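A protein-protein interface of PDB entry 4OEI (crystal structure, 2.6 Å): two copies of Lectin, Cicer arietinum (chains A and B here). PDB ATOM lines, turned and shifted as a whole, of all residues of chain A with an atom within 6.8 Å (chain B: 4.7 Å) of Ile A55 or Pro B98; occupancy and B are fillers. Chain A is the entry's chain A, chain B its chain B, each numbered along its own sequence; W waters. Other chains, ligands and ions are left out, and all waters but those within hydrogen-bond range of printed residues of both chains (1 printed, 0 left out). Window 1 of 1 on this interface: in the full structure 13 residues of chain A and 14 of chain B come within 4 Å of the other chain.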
ATOM      1  N   LEU A  51      24.030 -10.322  29.317  1.00  0.00           N
ATOM      2  CA  LEU A  51      24.711  -9.859  28.108  1.00  0.00           C
ATOM      3  C   LEU A  51      26.078  -9.203  28.360  1.00  0.00           C
ATOM      4  O   LEU A  51      26.713  -8.705  27.429  1.00  0.00           O
ATOM      5  CB  LEU A  51      23.821  -8.866  27.354  1.00  0.00           C
ATOM      6  CG  LEU A  51      22.366  -9.225  27.066  1.00  0.00           C
ATOM      7  CD1 LEU A  51      21.730  -8.121  26.224  1.00  0.00           C
ATOM      8  CD2 LEU A  51      22.298 -10.552  26.347  1.00  0.00           C
ATOM      9  N   ALA A  52      26.527  -9.211  29.613  1.00  0.00           N
ATOM     10  CA  ALA A  52      27.794  -8.594  29.983  1.00  0.00           C
ATOM     11  C   ALA A  52      28.994  -9.046  29.166  1.00  0.00           C
ATOM     12  O   ALA A  52      29.860  -8.231  28.843  1.00  0.00           O
ATOM     13  CB  ALA A  52      28.074  -8.823  31.458  1.00  0.00           C
ATOM     14  N   LYS A  53      29.054 -10.330  28.832  1.00  0.00           N
ATOM     15  CA  LYS A  53      30.186 -10.843  28.077  1.00  0.00           C
ATOM     16  C   LYS A  53      29.782 -11.335  26.698  1.00  0.00           C
ATOM     17  O   LYS A  53      30.154 -12.441  26.279  1.00  0.00           O
ATOM     18  CB  LYS A  53      30.856 -11.982  28.858  1.00  0.00           C
ATOM     19  CG  LYS A  53      31.058 -11.690  30.345  1.00  0.00           C
ATOM     20  CD  LYS A  53      31.822 -10.404  30.545  1.00  0.00           C
ATOM     21  CE  LYS A  53      33.150 -10.460  29.832  1.00  0.00           C
ATOM     22  NZ  LYS A  53      33.333  -9.249  28.984  1.00  0.00           N
ATOM     23  N   THR A  54      29.011 -10.517  25.994  1.00  0.00           N
ATOM     24  CA  THR A  54      28.548 -10.871  24.657  1.00  0.00           C
ATOM     25  C   THR A  54      28.809  -9.679  23.751  1.00  0.00           C
ATOM     26  O   THR A  54      29.183  -8.598  24.224  1.00  0.00           O
ATOM     27  CB  THR A  54      27.024 -11.139  24.641  1.00  0.00           C
ATOM     28  OG1 THR A  54      26.309  -9.936  24.982  1.00  0.00           O
ATOM     29  CG2 THR A  54      26.676 -12.225  25.642  1.00  0.00           C
ATOM     30  N   ILE A  55      28.604  -9.867  22.451  1.00  0.00           N
ATOM     31  CA  ILE A  55      28.822  -8.779  21.506  1.00  0.00           C
ATOM     32  C   ILE A  55      27.793  -7.672  21.735  1.00  0.00           C
ATOM     33  O   ILE A  55      28.057  -6.492  21.437  1.00  0.00           O
ATOM     34  CB  ILE A  55      28.740  -9.281  20.051  1.00  0.00           C
ATOM     35  CG1 ILE A  55      27.403 -10.006  19.825  1.00  0.00           C
ATOM     36  CG2 ILE A  55      29.912 -10.211  19.767  1.00  0.00           C
ATOM     37  CD1 ILE A  55      27.207 -10.521  18.404  1.00  0.00           C
ATOM     38  N   PHE A  56      26.635  -8.047  22.292  1.00  0.00           N
ATOM     39  CA  PHE A  56      25.540  -7.097  22.562  1.00  0.00           C
ATOM     40  C   PHE A  56      25.948  -6.195  23.725  1.00  0.00           C
ATOM     41  O   PHE A  56      25.622  -4.999  23.744  1.00  0.00           O
ATOM     42  CB  PHE A  56      24.264  -7.844  22.946  1.00  0.00           C
ATOM     43  CG  PHE A  56      23.834  -8.872  21.927  1.00  0.00           C
ATOM     44  CD1 PHE A  56      23.282  -8.494  20.702  1.00  0.00           C
ATOM     45  CD2 PHE A  56      23.954 -10.222  22.206  1.00  0.00           C
ATOM     46  CE1 PHE A  56      22.871  -9.454  19.783  1.00  0.00           C
ATOM     47  CE2 PHE A  56      23.549 -11.184  21.295  1.00  0.00           C
ATOM     48  CZ  PHE A  56      22.999 -10.805  20.089  1.00  0.00           C
ATOM     49  N   GLY A  57      26.650  -6.774  24.706  1.00  0.00           N
ATOM     50  CA  GLY A  57      27.101  -5.994  25.850  1.00  0.00           C
ATOM     51  C   GLY A  57      28.172  -5.021  25.400  1.00  0.00           C
ATOM     52  O   GLY A  57      28.296  -3.921  25.937  1.00  0.00           O
ATOM     53  N   THR A  58      28.942  -5.429  24.395  1.00  0.00           N
ATOM     54  CA  THR A  58      30.015  -4.602  23.857  1.00  0.00           C
ATOM     55  C   THR A  58      29.545  -3.493  22.908  1.00  0.00           C
ATOM     56  O   THR A  58      29.974  -2.344  23.029  1.00  0.00           O
ATOM     57  CB  THR A  58      31.036  -5.447  23.084  1.00  0.00           C
ATOM     58  OG1 THR A  58      31.579  -6.450  23.945  1.00  0.00           O
ATOM     59  CG2 THR A  58      32.158  -4.560  22.556  1.00  0.00           C
ATOM     60  N   TYR A  59      28.665  -3.828  21.971  1.00  0.00           N
ATOM     61  CA  TYR A  59      28.208  -2.839  20.992  1.00  0.00           C
ATOM     62  C   TYR A  59      26.749  -2.379  21.106  1.00  0.00           C
ATOM     63  O   TYR A  59      26.363  -1.377  20.500  1.00  0.00           O
ATOM     64  CB  TYR A  59      28.441  -3.383  19.582  1.00  0.00           C
ATOM     65  CG  TYR A  59      29.901  -3.611  19.281  1.00  0.00           C
ATOM     66  CD1 TYR A  59      30.789  -2.532  19.198  1.00  0.00           C
ATOM     67  CD2 TYR A  59      30.416  -4.907  19.160  1.00  0.00           C
ATOM     68  CE1 TYR A  59      32.153  -2.742  19.010  1.00  0.00           C
ATOM     69  CE2 TYR A  59      31.769  -5.125  18.976  1.00  0.00           C
ATOM     70  CZ  TYR A  59      32.630  -4.043  18.906  1.00  0.00           C
ATOM     71  OH  TYR A  59      33.971  -4.265  18.764  1.00  0.00           O
ATOM     72  N   GLY A  60      25.932  -3.096  21.865  1.00  0.00           N
ATOM     73  CA  GLY A  60      24.551  -2.683  21.985  1.00  0.00           C
ATOM     74  C   GLY A  60      23.637  -3.508  21.102  1.00  0.00           C
ATOM     75  O   GLY A  60      24.048  -4.526  20.536  1.00  0.00           O
ATOM     76  N   ILE A  61      22.392  -3.060  20.981  1.00  0.00           N
ATOM     77  CA  ILE A  61      21.392  -3.755  20.182  1.00  0.00           C
ATOM     78  C   ILE A  61      20.964  -2.835  19.039  1.00  0.00           C
ATOM     79  O   ILE A  61      20.614  -1.681  19.279  1.00  0.00           O
ATOM     80  CB  ILE A  61      20.167  -4.139  21.065  1.00  0.00           C
ATOM     81  CG1 ILE A  61      20.555  -5.249  22.062  1.00  0.00           C
ATOM     82  CG2 ILE A  61      19.039  -4.660  20.210  1.00  0.00           C
ATOM     83  CD1 ILE A  61      20.989  -4.764  23.419  1.00  0.00           C
ATOM     84  N   TYR A  76      22.326  -7.670  16.564  1.00  0.00           N
ATOM     85  CA  TYR A  76      23.494  -6.838  16.380  1.00  0.00           C
ATOM     86  C   TYR A  76      24.182  -7.346  15.136  1.00  0.00           C
ATOM     87  O   TYR A  76      24.839  -8.381  15.151  1.00  0.00           O
ATOM     88  CB  TYR A  76      24.467  -6.879  17.547  1.00  0.00           C
ATOM     89  CG  TYR A  76      25.592  -5.948  17.225  1.00  0.00           C
ATOM     90  CD1 TYR A  76      25.380  -4.563  17.182  1.00  0.00           C
ATOM     91  CD2 TYR A  76      26.820  -6.439  16.793  1.00  0.00           C
ATOM     92  CE1 TYR A  76      26.356  -3.697  16.706  1.00  0.00           C
ATOM     93  CE2 TYR A  76      27.802  -5.580  16.315  1.00  0.00           C
ATOM     94  CZ  TYR A  76      27.561  -4.215  16.273  1.00  0.00           C
ATOM     95  OH  TYR A  76      28.527  -3.380  15.786  1.00  0.00           O
ATOM     96  N   GLU A  77      24.010  -6.606  14.046  1.00  0.00           N
ATOM     97  CA  GLU A  77      24.565  -6.989  12.756  1.00  0.00           C
ATOM     98  C   GLU A  77      24.023  -8.389  12.447  1.00  0.00           C
ATOM     99  O   GLU A  77      22.877  -8.679  12.794  1.00  0.00           O
ATOM    100  CB  GLU A  77      26.091  -6.948  12.794  1.00  0.00           C
ATOM    101  CG  GLU A  77      26.611  -5.550  13.108  1.00  0.00           C
ATOM    102  CD  GLU A  77      28.105  -5.403  12.913  1.00  0.00           C
ATOM    103  OE1 GLU A  77      28.795  -6.441  12.817  1.00  0.00           O
ATOM    104  OE2 GLU A  77      28.583  -4.243  12.870  1.00  0.00           O
ATOM    105  N   ASN A  78      24.802  -9.272  11.838  1.00  0.00           N
ATOM    106  CA  ASN A  78      24.228 -10.575  11.510  1.00  0.00           C
ATOM    107  C   ASN A  78      23.884 -11.530  12.672  1.00  0.00           C
ATOM    108  O   ASN A  78      23.418 -12.649  12.434  1.00  0.00           O
ATOM    109  CB  ASN A  78      25.090 -11.295  10.447  1.00  0.00           C
ATOM    110  CG  ASN A  78      26.382 -11.877  11.011  1.00  0.00           C
ATOM    111  OD1 ASN A  78      26.437 -12.267  12.170  1.00  0.00           O
ATOM    112  ND2 ASN A  78      27.413 -11.972  10.175  1.00  0.00           N
ATOM    113  N   PHE A  79      24.080 -11.095  13.918  1.00  0.00           N
ATOM    114  CA  PHE A  79      23.778 -11.961  15.063  1.00  0.00           C
ATOM    115  C   PHE A  79      22.523 -11.555  15.845  1.00  0.00           C
ATOM    116  O   PHE A  79      22.125 -10.387  15.833  1.00  0.00           O
ATOM    117  CB  PHE A  79      24.981 -12.019  16.012  1.00  0.00           C
ATOM    118  CG  PHE A  79      26.210 -12.642  15.395  1.00  0.00           C
ATOM    119  CD1 PHE A  79      27.222 -11.847  14.860  1.00  0.00           C
ATOM    120  CD2 PHE A  79      26.353 -14.030  15.339  1.00  0.00           C
ATOM    121  CE1 PHE A  79      28.364 -12.422  14.274  1.00  0.00           C
ATOM    122  CE2 PHE A  79      27.484 -14.617  14.759  1.00  0.00           C
ATOM    123  CZ  PHE A  79      28.493 -13.813  14.228  1.00  0.00           C
ATOM    124  N   CYS A  80      21.896 -12.518  16.518  1.00  0.00           N
ATOM    125  CA  CYS A  80      20.688 -12.245  17.301  1.00  0.00           C
ATOM    126  C   CYS A  80      20.521 -13.268  18.414  1.00  0.00           C
ATOM    127  O   CYS A  80      21.222 -14.275  18.450  1.00  0.00           O
ATOM    128  CB  CYS A  80      19.452 -12.296  16.400  1.00  0.00           C
ATOM    129  SG  CYS A  80      19.128 -13.943  15.706  1.00  0.00           S
ATOM    130  N   PRO A  98      23.551 -16.904  21.402  1.00  0.00           N
ATOM    131  CA  PRO A  98      23.345 -16.163  20.158  1.00  0.00           C
ATOM    132  C   PRO A  98      23.725 -16.936  18.908  1.00  0.00           C
ATOM    133  O   PRO A  98      24.677 -17.704  18.913  1.00  0.00           O
ATOM    134  CB  PRO A  98      24.236 -14.948  20.356  1.00  0.00           C
ATOM    135  CG  PRO A  98      25.442 -15.578  20.996  1.00  0.00           C
ATOM    136  CD  PRO A  98      24.820 -16.504  22.038  1.00  0.00           C
ATOM    137  N   ILE B  55      28.966 -16.173  20.798  1.00  0.00           N
ATOM    138  CA  ILE B  55      29.061 -16.722  19.445  1.00  0.00           C
ATOM    139  C   ILE B  55      30.125 -17.812  19.327  1.00  0.00           C
ATOM    140  O   ILE B  55      29.984 -18.747  18.519  1.00  0.00           O
ATOM    141  CB  ILE B  55      29.377 -15.627  18.431  1.00  0.00           C
ATOM    142  CG1 ILE B  55      30.636 -14.882  18.880  1.00  0.00           C
ATOM    143  CG2 ILE B  55      28.200 -14.679  18.330  1.00  0.00           C
ATOM    144  CD1 ILE B  55      31.111 -13.821  17.913  1.00  0.00           C
ATOM    145  N   PHE B  56      31.181 -17.694  20.137  1.00  0.00           N
ATOM    146  CA  PHE B  56      32.271 -18.674  20.134  1.00  0.00           C
ATOM    147  C   PHE B  56      31.720 -20.019  20.604  1.00  0.00           C
ATOM    148  O   PHE B  56      32.136 -21.081  20.113  1.00  0.00           O
ATOM    149  CB  PHE B  56      33.398 -18.232  21.075  1.00  0.00           C
ATOM    150  CG  PHE B  56      34.022 -16.927  20.684  1.00  0.00           C
ATOM    151  CD1 PHE B  56      34.641 -16.784  19.449  1.00  0.00           C
ATOM    152  CD2 PHE B  56      33.965 -15.828  21.538  1.00  0.00           C
ATOM    153  CE1 PHE B  56      35.182 -15.569  19.063  1.00  0.00           C
ATOM    154  CE2 PHE B  56      34.502 -14.601  21.164  1.00  0.00           C
ATOM    155  CZ  PHE B  56      35.119 -14.468  19.921  1.00  0.00           C
ATOM    156  N   PHE B  79      34.902 -11.221  14.888  1.00  0.00           N
ATOM    157  CA  PHE B  79      35.108 -11.146  16.333  1.00  0.00           C
ATOM    158  C   PHE B  79      36.238 -11.920  17.018  1.00  0.00           C
ATOM    159  O   PHE B  79      36.646 -13.001  16.580  1.00  0.00           O
ATOM    160  CB  PHE B  79      33.776 -11.474  17.020  1.00  0.00           C
ATOM    161  CG  PHE B  79      32.646 -10.569  16.597  1.00  0.00           C
ATOM    162  CD1 PHE B  79      31.850 -10.881  15.494  1.00  0.00           C
ATOM    163  CD2 PHE B  79      32.433  -9.357  17.256  1.00  0.00           C
ATOM    164  CE1 PHE B  79      30.857  -9.998  15.053  1.00  0.00           C
ATOM    165  CE2 PHE B  79      31.445  -8.467  16.822  1.00  0.00           C
ATOM    166  CZ  PHE B  79      30.658  -8.787  15.716  1.00  0.00           C
ATOM    167  N   CYS B  80      36.725 -11.357  18.119  1.00  0.00           N
ATOM    168  CA  CYS B  80      37.806 -11.963  18.892  1.00  0.00           C
ATOM    169  C   CYS B  80      37.611 -11.684  20.375  1.00  0.00           C
ATOM    170  O   CYS B  80      36.741 -10.910  20.758  1.00  0.00           O
ATOM    171  CB  CYS B  80      39.151 -11.388  18.451  1.00  0.00           C
ATOM    172  SG  CYS B  80      39.295  -9.594  18.696  1.00  0.00           S
ATOM    173  N   ALA B  81      38.427 -12.317  21.206  1.00  0.00           N
ATOM    174  CA  ALA B  81      38.346 -12.113  22.647  1.00  0.00           C
ATOM    175  C   ALA B  81      39.633 -12.565  23.312  1.00  0.00           C
ATOM    176  O   ALA B  81      40.382 -13.360  22.742  1.00  0.00           O
ATOM    177  CB  ALA B  81      37.153 -12.897  23.230  1.00  0.00           C
ATOM    178  N   SER B  96      38.915  -9.672  27.841  1.00  0.00           N
ATOM    179  CA  SER B  96      38.552  -8.558  26.958  1.00  0.00           C
ATOM    180  C   SER B  96      37.595  -9.131  25.907  1.00  0.00           C
ATOM    181  O   SER B  96      37.748 -10.279  25.487  1.00  0.00           O
ATOM    182  CB  SER B  96      39.785  -7.972  26.252  1.00  0.00           C
ATOM    183  OG  SER B  96      40.504  -7.061  27.091  1.00  0.00           O
ATOM    184  N   GLY B  97      36.596  -8.353  25.507  1.00  0.00           N
ATOM    185  CA  GLY B  97      35.665  -8.813  24.485  1.00  0.00           C
ATOM    186  C   GLY B  97      34.398  -9.522  24.930  1.00  0.00           C
ATOM    187  O   GLY B  97      34.103  -9.588  26.125  1.00  0.00           O
ATOM    188  N   PRO B  98      33.625 -10.081  23.978  1.00  0.00           N
ATOM    189  CA  PRO B  98      33.887 -10.096  22.532  1.00  0.00           C
ATOM    190  C   PRO B  98      33.846  -8.736  21.845  1.00  0.00           C
ATOM    191  O   PRO B  98      32.923  -7.963  22.065  1.00  0.00           O
ATOM    192  CB  PRO B  98      32.779 -10.997  21.978  1.00  0.00           C
ATOM    193  CG  PRO B  98      32.342 -11.820  23.164  1.00  0.00           C
ATOM    194  CD  PRO B  98      32.393 -10.826  24.284  1.00  0.00           C
ATOM    195  N   LYS B  99      34.850  -8.455  21.018  1.00  0.00           N
ATOM    196  CA  LYS B  99      34.881  -7.223  20.243  1.00  0.00           C
ATOM    197  C   LYS B  99      35.414  -7.539  18.861  1.00  0.00           C
ATOM    198  O   LYS B  99      35.995  -8.600  18.614  1.00  0.00           O
ATOM    199  CB  LYS B  99      35.747  -6.115  20.869  1.00  0.00           C
ATOM    200  CG  LYS B  99      36.633  -6.523  22.035  1.00  0.00           C
ATOM    201  CD  LYS B  99      37.902  -5.670  22.104  1.00  0.00           C
ATOM    202  CE  LYS B  99      37.664  -4.275  22.664  1.00  0.00           C
ATOM    203  NZ  LYS B  99      37.399  -4.305  24.137  1.00  0.00           N
ATOM    204  N   LYS B 100      35.185  -6.609  17.948  1.00  0.00           N
ATOM    205  CA  LYS B 100      35.639  -6.757  16.587  1.00  0.00           C
ATOM    206  C   LYS B 100      37.155  -6.778  16.565  1.00  0.00           C
ATOM    207  O   LYS B 100      37.806  -6.226  17.466  1.00  0.00           O
ATOM    208  CB  LYS B 100      35.156  -5.580  15.769  1.00  0.00           C
ATOM    209  CG  LYS B 100      33.777  -5.765  15.284  1.00  0.00           C
ATOM    210  CD  LYS B 100      33.111  -4.450  15.093  1.00  0.00           C
ATOM    211  CE  LYS B 100      31.866  -4.672  14.263  1.00  0.00           C
ATOM    212  NZ  LYS B 100      30.943  -3.514  14.336  1.00  0.00           N
HETATM  213  O   HOH W   1      28.801 -13.142  21.803  1.00  0.00           O
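The side-chain amino group (NZ) of Lys A53 lies within hydrogen-bond range of the backbone carbonyl oxygen (O) of Gly B97. NZ of Lys B100 is in hydrogen-bond range of OH of Tyr A76 (2.8 Å). OH of Tyr A59 is in hydrogen-bond range of N of Lys B100 (2.8 Å). OG1 of Thr A58 lies within hydrogen-bond range of O of Pro B98 (2.8 Å). The side-chain amino group of Lys B100 is in salt-bridge range of the side-chain carboxylate of Glu A77 (2.9 Å).
The side-chain hydroxyl (OG1) of Thr A54 lies close to the backbone NH (N) of Phe A56, 3.3 Å away. The side-chain hydroxyl of Tyr A76 is in hydrogen-bond range of the side-chain carboxylate of Glu A77. The backbone carbonyl oxygen of Leu A51 lies within hydrogen-bond range of the side-chain hydroxyl of Thr A54, 2.8 Å away. OG1 of Thr A58 sits at hydrogen-bond distance from O of Thr A54 (3.2 Å). OG1 of Thr A54 sits at hydrogen-bond distance from N of Gly A57, 3.2 Å away. The backbone NH (N) of Cys B80 sits at hydrogen-bond distance from the backbone carbonyl oxygen (O) of Lys B99 (2.9 Å).
CD of Pro B98 touches O of Lys A53 (3.4 Å). CD of Pro B98 touches C of Thr A54, at 3.8 Å. Ile A55 touches Phe B79. Pro B98 touches Ile A55. Phe B79 touches Tyr A59. CB of Lys B99 touches OH of Tyr A59, 3.3 Å away. CD2 of Phe A79 touches CG2 of Ile B55, 3.6 Å away. CE1 of Phe A79 touches CE1 of Phe B79 (3.6 Å). N of Ile B55 touches CG of Pro A98 (3.6 Å).
Ile A55 touches just these residues of chain B: Phe B79 (3.7 Å) and Pro B98 (3.7 Å). Of the printed residues of chain B, Thr A58 touches Pro B98 (2.8 Å). Of the printed residues of chain B, Tyr A59 touches Phe B79, Lys B99 and Lys B100. Ile A61 touches none of the printed residues of chain B. Printed residues of chain B within 4 Å of Glu A77: Lys B100 (2.9 Å). Of the printed residues of chain A, Ile B55 touches Phe A79 and Pro A98. Of the printed residues of chain A, Pro B98 touches Lys A53, Thr A54, Ile A55 and Thr A58. Of the printed residues of chain A, Lys B99 touches Tyr A59 (3.3 Å). The nearest residue of chain B that does not touch Ile A55 is Ile B55 (4.2 Å). The nearest residue of chain A that does not touch Pro B98 is Tyr A59 (4.4 Å).
Hydrophobic or aromatic side chains of chain A that line the printed part of chain B: Ile A55, Tyr A59, Tyr A76, Phe A79 and Pro A98. Printed residues of chain B that touch a printed residue of chain A: Ile B55, Phe B79, Gly B97, Pro B98, Lys B99 and Lys B100.
Ile A55 touches Phe B79, and with the chains exchanged Phe A79 touches Ile B55. Ile A55 touches Pro B98, and with the chains exchanged Pro A98 touches Ile B55. Phe A79 touches its own counterpart, Phe B79. Positions printed for both chains: 55, 56, 79, 80 and 98.
Water W1 lies within hydrogen-bond range of the backbone NH of Ile B55 (3.2 Å) and the backbone NH of Ile A55 (3.3 Å).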
